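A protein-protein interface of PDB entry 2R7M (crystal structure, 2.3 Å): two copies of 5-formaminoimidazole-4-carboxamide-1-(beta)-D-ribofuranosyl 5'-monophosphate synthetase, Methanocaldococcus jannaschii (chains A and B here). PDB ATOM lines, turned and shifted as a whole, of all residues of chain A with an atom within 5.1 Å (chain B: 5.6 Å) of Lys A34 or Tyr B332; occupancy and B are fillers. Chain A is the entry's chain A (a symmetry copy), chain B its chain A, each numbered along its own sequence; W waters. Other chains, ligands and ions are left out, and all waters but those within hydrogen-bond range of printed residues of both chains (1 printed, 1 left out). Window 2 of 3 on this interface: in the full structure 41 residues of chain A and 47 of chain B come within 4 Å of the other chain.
NZ of Lys A34 sits at hydrogen-bond distance from O of Leu B331.
O of Leu B222 lies within hydrogen-bond range of OH of Tyr B332 (2.9 Å).
Among the printed residues, pairs that only touch across the chains: Arg A57 with Tyr B332 (3.3 Å), Phe A58 with Tyr B332 (3.5 Å), Phe A58 with Tyr B328 (3.5 Å), Phe A58 with Leu B222 (3.7 Å), Phe A58 with Phe B272 (3.7 Å), Lys A34 with Gly B334 (3.7 Å), Phe A58 with Leu B331 (3.7 Å), Leu A30 with Leu B331 (3.8 Å), Arg A57 with Phe B272 (3.8 Å) and Lys A34 with Tyr B332 (3.8 Å).
Of the printed residues of chain B, Lys A34 touches Leu B331 (2.7 Å), Tyr B332 (3.8 Å) and Gly B334 (3.7 Å).
Tyr B332 touches just these residues of chain A: Lys A34 (3.8 Å), Arg A57 (3.3 Å) and Phe A58 (3.5 Å).
Printed residues of chain A within 4 Å of Phe B272: Arg A57 (3.8 Å) and Phe A58 (3.7 Å).
Of the printed residues of chain B, Leu A30 touches Leu B331.
Of the printed residues of chain A, Tyr B328 touches Phe A58 (3.5 Å).
Printed residues of chain A within 4 Å of Leu B222: Phe A58.
Val A60 touches none of the printed residues of chain B.
The nearest printed residue of chain A that does not touch Tyr B332 is Val A60 (6.6 Å).
Hydrophobic or aromatic side chains of chain A within 4 Å of the printed part of chain B: Leu A30 and Phe A58.
Among the printed residues, 11 pairs touch across the chains.
No position is printed for both chains.
Water W1 lies within hydrogen-bond range of NZ of Lys A34 and O of Asn B333.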
ATOM      1  N   SER A  29      28.500 -22.874 -13.264  1.00  0.00           N
ATOM      2  CA  SER A  29      28.715 -24.281 -12.930  1.00  0.00           C
ATOM      3  C   SER A  29      27.645 -24.858 -12.006  1.00  0.00           C
ATOM      4  O   SER A  29      27.445 -26.059 -11.969  1.00  0.00           O
ATOM      5  CB  SER A  29      30.101 -24.493 -12.321  1.00  0.00           C
ATOM      6  OG  SER A  29      30.162 -23.922 -11.026  1.00  0.00           O
ATOM      7  N   LEU A  30      26.966 -23.998 -11.257  1.00  0.00           N
ATOM      8  CA  LEU A  30      25.890 -24.443 -10.377  1.00  0.00           C
ATOM      9  C   LEU A  30      24.765 -25.187 -11.108  1.00  0.00           C
ATOM     10  O   LEU A  30      24.285 -26.199 -10.608  1.00  0.00           O
ATOM     11  CB  LEU A  30      25.309 -23.273  -9.585  1.00  0.00           C
ATOM     12  CG  LEU A  30      26.138 -22.753  -8.413  1.00  0.00           C
ATOM     13  CD1 LEU A  30      25.382 -21.628  -7.723  1.00  0.00           C
ATOM     14  CD2 LEU A  30      26.441 -23.880  -7.440  1.00  0.00           C
ATOM     15  N   HIS A  31      24.346 -24.692 -12.269  1.00  0.00           N
ATOM     16  CA  HIS A  31      23.293 -25.361 -13.046  1.00  0.00           C
ATOM     17  C   HIS A  31      23.845 -26.360 -14.062  1.00  0.00           C
ATOM     18  O   HIS A  31      23.143 -27.291 -14.455  1.00  0.00           O
ATOM     19  CB  HIS A  31      22.300 -24.373 -13.690  1.00  0.00           C
ATOM     20  CG  HIS A  31      22.890 -23.497 -14.753  1.00  0.00           C
ATOM     21  ND1 HIS A  31      22.906 -23.852 -16.085  1.00  0.00           N
ATOM     22  CD2 HIS A  31      23.456 -22.269 -14.685  1.00  0.00           C
ATOM     23  CE1 HIS A  31      23.476 -22.892 -16.790  1.00  0.00           C
ATOM     24  NE2 HIS A  31      23.800 -21.910 -15.967  1.00  0.00           N
ATOM     25  N   ILE A  32      25.100 -26.172 -14.475  1.00  0.00           N
ATOM     26  CA  ILE A  32      25.811 -27.188 -15.234  1.00  0.00           C
ATOM     27  C   ILE A  32      25.894 -28.485 -14.414  1.00  0.00           C
ATOM     28  O   ILE A  32      25.626 -29.577 -14.927  1.00  0.00           O
ATOM     29  CB  ILE A  32      27.252 -26.743 -15.609  1.00  0.00           C
ATOM     30  CG1 ILE A  32      27.225 -25.664 -16.698  1.00  0.00           C
ATOM     31  CG2 ILE A  32      28.086 -27.933 -16.091  1.00  0.00           C
ATOM     32  CD1 ILE A  32      28.548 -24.922 -16.847  1.00  0.00           C
ATOM     33  N   LEU A  33      26.259 -28.352 -13.141  1.00  0.00           N
ATOM     34  CA  LEU A  33      26.416 -29.501 -12.263  1.00  0.00           C
ATOM     35  C   LEU A  33      25.075 -30.012 -11.724  1.00  0.00           C
ATOM     36  O   LEU A  33      24.861 -31.222 -11.636  1.00  0.00           O
ATOM     37  CB  LEU A  33      27.402 -29.190 -11.128  1.00  0.00           C
ATOM     38  CG  LEU A  33      28.852 -28.909 -11.558  1.00  0.00           C
ATOM     39  CD1 LEU A  33      29.731 -28.648 -10.349  1.00  0.00           C
ATOM     40  CD2 LEU A  33      29.441 -30.039 -12.419  1.00  0.00           C
ATOM     41  N   LYS A  34      24.179 -29.097 -11.363  1.00  0.00           N
ATOM     42  CA  LYS A  34      22.815 -29.485 -11.007  1.00  0.00           C
ATOM     43  C   LYS A  34      22.117 -30.178 -12.163  1.00  0.00           C
ATOM     44  O   LYS A  34      21.512 -31.233 -11.987  1.00  0.00           O
ATOM     45  CB  LYS A  34      21.981 -28.288 -10.557  1.00  0.00           C
ATOM     46  CG  LYS A  34      20.575 -28.666 -10.100  1.00  0.00           C
ATOM     47  CD  LYS A  34      20.625 -29.468  -8.811  1.00  0.00           C
ATOM     48  CE  LYS A  34      19.256 -30.047  -8.467  1.00  0.00           C
ATOM     49  NZ  LYS A  34      19.273 -30.738  -7.165  1.00  0.00           N
ATOM     50  N   GLY A  35      22.204 -29.581 -13.347  1.00  0.00           N
ATOM     51  CA  GLY A  35      21.582 -30.157 -14.530  1.00  0.00           C
ATOM     52  C   GLY A  35      22.082 -31.554 -14.839  1.00  0.00           C
ATOM     53  O   GLY A  35      21.321 -32.419 -15.272  1.00  0.00           O
ATOM     54  N   ALA A  36      23.377 -31.768 -14.628  1.00  0.00           N
ATOM     55  CA  ALA A  36      23.991 -33.081 -14.800  1.00  0.00           C
ATOM     56  C   ALA A  36      23.423 -34.123 -13.822  1.00  0.00           C
ATOM     57  O   ALA A  36      23.016 -35.203 -14.234  1.00  0.00           O
ATOM     58  CB  ALA A  36      25.491 -32.972 -14.644  1.00  0.00           C
ATOM     59  N   LYS A  37      23.398 -33.796 -12.534  1.00  0.00           N
ATOM     60  CA  LYS A  37      22.827 -34.687 -11.530  1.00  0.00           C
ATOM     61  C   LYS A  37      21.399 -35.091 -11.907  1.00  0.00           C
ATOM     62  O   LYS A  37      21.045 -36.264 -11.831  1.00  0.00           O
ATOM     63  CB  LYS A  37      22.825 -34.022 -10.148  1.00  0.00           C
ATOM     64  CG  LYS A  37      24.202 -33.765  -9.539  1.00  0.00           C
ATOM     65  CD  LYS A  37      24.778 -34.992  -8.875  1.00  0.00           C
ATOM     66  CE  LYS A  37      24.019 -35.351  -7.609  1.00  0.00           C
ATOM     67  NZ  LYS A  37      24.778 -36.333  -6.788  1.00  0.00           N
ATOM     68  N   LEU A  38      20.594 -34.111 -12.320  1.00  0.00           N
ATOM     69  CA  LEU A  38      19.193 -34.318 -12.698  1.00  0.00           C
ATOM     70  C   LEU A  38      19.059 -35.277 -13.869  1.00  0.00           C
ATOM     71  O   LEU A  38      18.027 -35.927 -14.019  1.00  0.00           O
ATOM     72  CB  LEU A  38      18.509 -32.982 -13.055  1.00  0.00           C
ATOM     73  CG  LEU A  38      18.249 -31.985 -11.913  1.00  0.00           C
ATOM     74  CD1 LEU A  38      17.910 -30.616 -12.465  1.00  0.00           C
ATOM     75  CD2 LEU A  38      17.143 -32.463 -10.975  1.00  0.00           C
ATOM     76  N   ARG A  57      27.635 -26.367  -0.317  1.00  0.00           N
ATOM     77  CA  ARG A  57      26.365 -26.123   0.354  1.00  0.00           C
ATOM     78  C   ARG A  57      25.177 -26.328  -0.579  1.00  0.00           C
ATOM     79  O   ARG A  57      24.063 -26.592  -0.135  1.00  0.00           O
ATOM     80  CB  ARG A  57      26.348 -24.743   1.015  1.00  0.00           C
ATOM     81  CG  ARG A  57      27.492 -24.548   2.002  1.00  0.00           C
ATOM     82  CD  ARG A  57      27.114 -23.649   3.167  1.00  0.00           C
ATOM     83  NE  ARG A  57      28.272 -23.368   4.007  1.00  0.00           N
ATOM     84  CZ  ARG A  57      28.469 -22.234   4.680  1.00  0.00           C
ATOM     85  NH1 ARG A  57      27.585 -21.247   4.615  1.00  0.00           N
ATOM     86  NH2 ARG A  57      29.567 -22.081   5.408  1.00  0.00           N
ATOM     87  N   PHE A  58      25.416 -26.232  -1.875  1.00  0.00           N
ATOM     88  CA  PHE A  58      24.357 -26.483  -2.830  1.00  0.00           C
ATOM     89  C   PHE A  58      24.291 -27.975  -3.203  1.00  0.00           C
ATOM     90  O   PHE A  58      23.370 -28.393  -3.896  1.00  0.00           O
ATOM     91  CB  PHE A  58      24.501 -25.566  -4.055  1.00  0.00           C
ATOM     92  CG  PHE A  58      23.946 -24.173  -3.840  1.00  0.00           C
ATOM     93  CD1 PHE A  58      22.647 -23.991  -3.374  1.00  0.00           C
ATOM     94  CD2 PHE A  58      24.715 -23.049  -4.115  1.00  0.00           C
ATOM     95  CE1 PHE A  58      22.126 -22.709  -3.188  1.00  0.00           C
ATOM     96  CE2 PHE A  58      24.199 -21.762  -3.932  1.00  0.00           C
ATOM     97  CZ  PHE A  58      22.912 -21.589  -3.471  1.00  0.00           C
ATOM     98  N   VAL A  60      26.050 -30.012  -5.115  1.00  0.00           N
ATOM     99  CA  VAL A  60      25.851 -30.114  -6.541  1.00  0.00           C
ATOM    100  C   VAL A  60      26.994 -30.889  -7.197  1.00  0.00           C
ATOM    101  O   VAL A  60      26.917 -31.279  -8.363  1.00  0.00           O
ATOM    102  CB  VAL A  60      25.626 -28.672  -7.116  1.00  0.00           C
ATOM    103  CG1 VAL A  60      26.859 -28.111  -7.810  1.00  0.00           C
ATOM    104  CG2 VAL A  60      24.398 -28.630  -7.992  1.00  0.00           C
ATOM    105  N   GLU B 221      22.613 -21.016   4.634  1.00  0.00           N
ATOM    106  CA  GLU B 221      22.154 -21.399   3.290  1.00  0.00           C
ATOM    107  C   GLU B 221      21.784 -20.146   2.492  1.00  0.00           C
ATOM    108  O   GLU B 221      21.278 -19.186   3.063  1.00  0.00           O
ATOM    109  CB  GLU B 221      20.901 -22.297   3.403  1.00  0.00           C
ATOM    110  CG  GLU B 221      21.152 -23.639   4.091  1.00  0.00           C
ATOM    111  CD  GLU B 221      19.889 -24.307   4.611  1.00  0.00           C
ATOM    112  OE1 GLU B 221      18.762 -23.876   4.275  1.00  0.00           O
ATOM    113  OE2 GLU B 221      20.026 -25.279   5.370  1.00  0.00           O
ATOM    114  N   LEU B 222      22.015 -20.165   1.183  1.00  0.00           N
ATOM    115  CA  LEU B 222      21.499 -19.120   0.301  1.00  0.00           C
ATOM    116  C   LEU B 222      20.160 -19.544  -0.325  1.00  0.00           C
ATOM    117  O   LEU B 222      20.066 -20.580  -0.991  1.00  0.00           O
ATOM    118  CB  LEU B 222      22.526 -18.775  -0.781  1.00  0.00           C
ATOM    119  CG  LEU B 222      22.136 -17.776  -1.877  1.00  0.00           C
ATOM    120  CD1 LEU B 222      21.682 -16.426  -1.319  1.00  0.00           C
ATOM    121  CD2 LEU B 222      23.316 -17.596  -2.793  1.00  0.00           C
ATOM    122  N   LEU B 223      19.123 -18.747  -0.101  1.00  0.00           N
ATOM    123  CA  LEU B 223      17.775 -19.099  -0.563  1.00  0.00           C
ATOM    124  C   LEU B 223      17.342 -18.327  -1.800  1.00  0.00           C
ATOM    125  O   LEU B 223      16.668 -18.873  -2.685  1.00  0.00           O
ATOM    126  CB  LEU B 223      16.744 -18.924   0.567  1.00  0.00           C
ATOM    127  CG  LEU B 223      16.452 -20.164   1.435  1.00  0.00           C
ATOM    128  CD1 LEU B 223      15.726 -21.225   0.646  1.00  0.00           C
ATOM    129  CD2 LEU B 223      17.714 -20.751   2.055  1.00  0.00           C
ATOM    130  N   PHE B 272      28.556 -15.954   0.697  1.00  0.00           N
ATOM    131  CA  PHE B 272      28.449 -16.902   1.812  1.00  0.00           C
ATOM    132  C   PHE B 272      29.304 -16.469   3.012  1.00  0.00           C
ATOM    133  O   PHE B 272      28.863 -16.549   4.171  1.00  0.00           O
ATOM    134  CB  PHE B 272      28.851 -18.311   1.358  1.00  0.00           C
ATOM    135  CG  PHE B 272      27.789 -19.040   0.560  1.00  0.00           C
ATOM    136  CD1 PHE B 272      27.839 -19.076  -0.828  1.00  0.00           C
ATOM    137  CD2 PHE B 272      26.756 -19.711   1.201  1.00  0.00           C
ATOM    138  CE1 PHE B 272      26.870 -19.754  -1.566  1.00  0.00           C
ATOM    139  CE2 PHE B 272      25.786 -20.392   0.472  1.00  0.00           C
ATOM    140  CZ  PHE B 272      25.847 -20.418  -0.908  1.00  0.00           C
ATOM    141  N   TYR B 328      18.228 -20.152  -6.914  1.00  0.00           N
ATOM    142  CA  TYR B 328      19.059 -20.704  -5.842  1.00  0.00           C
ATOM    143  C   TYR B 328      18.310 -21.732  -4.968  1.00  0.00           C
ATOM    144  O   TYR B 328      18.883 -22.741  -4.600  1.00  0.00           O
ATOM    145  CB  TYR B 328      19.680 -19.588  -4.965  1.00  0.00           C
ATOM    146  CG  TYR B 328      20.574 -18.638  -5.733  1.00  0.00           C
ATOM    147  CD1 TYR B 328      21.808 -19.055  -6.206  1.00  0.00           C
ATOM    148  CD2 TYR B 328      20.169 -17.327  -6.010  1.00  0.00           C
ATOM    149  CE1 TYR B 328      22.625 -18.205  -6.930  1.00  0.00           C
ATOM    150  CE2 TYR B 328      20.989 -16.457  -6.737  1.00  0.00           C
ATOM    151  CZ  TYR B 328      22.210 -16.905  -7.189  1.00  0.00           C
ATOM    152  OH  TYR B 328      23.023 -16.080  -7.917  1.00  0.00           O
ATOM    153  N   SER B 329      17.042 -21.476  -4.640  1.00  0.00           N
ATOM    154  CA  SER B 329      16.291 -22.404  -3.781  1.00  0.00           C
ATOM    155  C   SER B 329      16.089 -23.757  -4.467  1.00  0.00           C
ATOM    156  O   SER B 329      15.941 -24.777  -3.803  1.00  0.00           O
ATOM    157  CB  SER B 329      14.967 -21.800  -3.275  1.00  0.00           C
ATOM    158  OG  SER B 329      13.978 -21.750  -4.286  1.00  0.00           O
ATOM    159  N   PHE B 330      16.164 -23.743  -5.797  1.00  0.00           N
ATOM    160  CA  PHE B 330      16.011 -24.921  -6.651  1.00  0.00           C
ATOM    161  C   PHE B 330      17.163 -25.929  -6.562  1.00  0.00           C
ATOM    162  O   PHE B 330      16.959 -27.127  -6.767  1.00  0.00           O
ATOM    163  CB  PHE B 330      15.869 -24.465  -8.105  1.00  0.00           C
ATOM    164  CG  PHE B 330      15.667 -25.585  -9.084  1.00  0.00           C
ATOM    165  CD1 PHE B 330      14.414 -26.152  -9.255  1.00  0.00           C
ATOM    166  CD2 PHE B 330      16.725 -26.063  -9.841  1.00  0.00           C
ATOM    167  CE1 PHE B 330      14.230 -27.178 -10.142  1.00  0.00           C
ATOM    168  CE2 PHE B 330      16.539 -27.093 -10.735  1.00  0.00           C
ATOM    169  CZ  PHE B 330      15.294 -27.650 -10.882  1.00  0.00           C
ATOM    170  N   LEU B 331      18.374 -25.442  -6.291  1.00  0.00           N
ATOM    171  CA  LEU B 331      19.574 -26.260  -6.427  1.00  0.00           C
ATOM    172  C   LEU B 331      19.613 -27.412  -5.418  1.00  0.00           C
ATOM    173  O   LEU B 331      20.042 -28.508  -5.752  1.00  0.00           O
ATOM    174  CB  LEU B 331      20.843 -25.400  -6.312  1.00  0.00           C
ATOM    175  CG  LEU B 331      21.594 -24.813  -7.526  1.00  0.00           C
ATOM    176  CD1 LEU B 331      20.845 -24.883  -8.860  1.00  0.00           C
ATOM    177  CD2 LEU B 331      22.072 -23.384  -7.233  1.00  0.00           C
ATOM    178  N   TYR B 332      19.177 -27.141  -4.191  1.00  0.00           N
ATOM    179  CA  TYR B 332      19.080 -28.135  -3.123  1.00  0.00           C
ATOM    180  C   TYR B 332      18.421 -29.463  -3.503  1.00  0.00           C
ATOM    181  O   TYR B 332      19.024 -30.528  -3.333  1.00  0.00           O
ATOM    182  CB  TYR B 332      18.383 -27.535  -1.894  1.00  0.00           C
ATOM    183  CG  TYR B 332      19.111 -26.334  -1.347  1.00  0.00           C
ATOM    184  CD1 TYR B 332      20.363 -26.473  -0.753  1.00  0.00           C
ATOM    185  CD2 TYR B 332      18.572 -25.053  -1.461  1.00  0.00           C
ATOM    186  CE1 TYR B 332      21.047 -25.372  -0.258  1.00  0.00           C
ATOM    187  CE2 TYR B 332      19.251 -23.938  -0.974  1.00  0.00           C
ATOM    188  CZ  TYR B 332      20.484 -24.110  -0.371  1.00  0.00           C
ATOM    189  OH  TYR B 332      21.165 -23.023   0.111  1.00  0.00           O
ATOM    190  N   ASN B 333      17.188 -29.403  -4.006  1.00  0.00           N
ATOM    191  CA  ASN B 333      16.424 -30.623  -4.291  1.00  0.00           C
ATOM    192  C   ASN B 333      15.562 -30.553  -5.541  1.00  0.00           C
ATOM    193  O   ASN B 333      14.637 -31.344  -5.694  1.00  0.00           O
ATOM    194  CB  ASN B 333      15.540 -30.977  -3.092  1.00  0.00           C
ATOM    195  CG  ASN B 333      16.347 -31.406  -1.877  1.00  0.00           C
ATOM    196  OD1 ASN B 333      17.137 -32.340  -1.951  1.00  0.00           O
ATOM    197  ND2 ASN B 333      16.155 -30.720  -0.758  1.00  0.00           N
ATOM    198  N   GLY B 334      15.838 -29.591  -6.418  1.00  0.00           N
ATOM    199  CA  GLY B 334      15.037 -29.405  -7.626  1.00  0.00           C
ATOM    200  C   GLY B 334      13.585 -29.044  -7.355  1.00  0.00           C
ATOM    201  O   GLY B 334      12.692 -29.353  -8.154  1.00  0.00           O
ATOM    202  N   LEU B 337      11.068 -24.206  -3.898  1.00  0.00           N
ATOM    203  CA  LEU B 337      11.159 -23.933  -2.461  1.00  0.00           C
ATOM    204  C   LEU B 337      11.156 -22.436  -2.118  1.00  0.00           C
ATOM    205  O   LEU B 337      12.054 -21.701  -2.530  1.00  0.00           O
ATOM    206  CB  LEU B 337      12.440 -24.588  -1.912  1.00  0.00           C
ATOM    207  CG  LEU B 337      12.856 -24.374  -0.451  1.00  0.00           C
ATOM    208  CD1 LEU B 337      11.994 -25.158   0.526  1.00  0.00           C
ATOM    209  CD2 LEU B 337      14.306 -24.753  -0.279  1.00  0.00           C
HETATM  210  O   HOH W   1      17.571 -32.838  -6.740  1.00  0.00           O
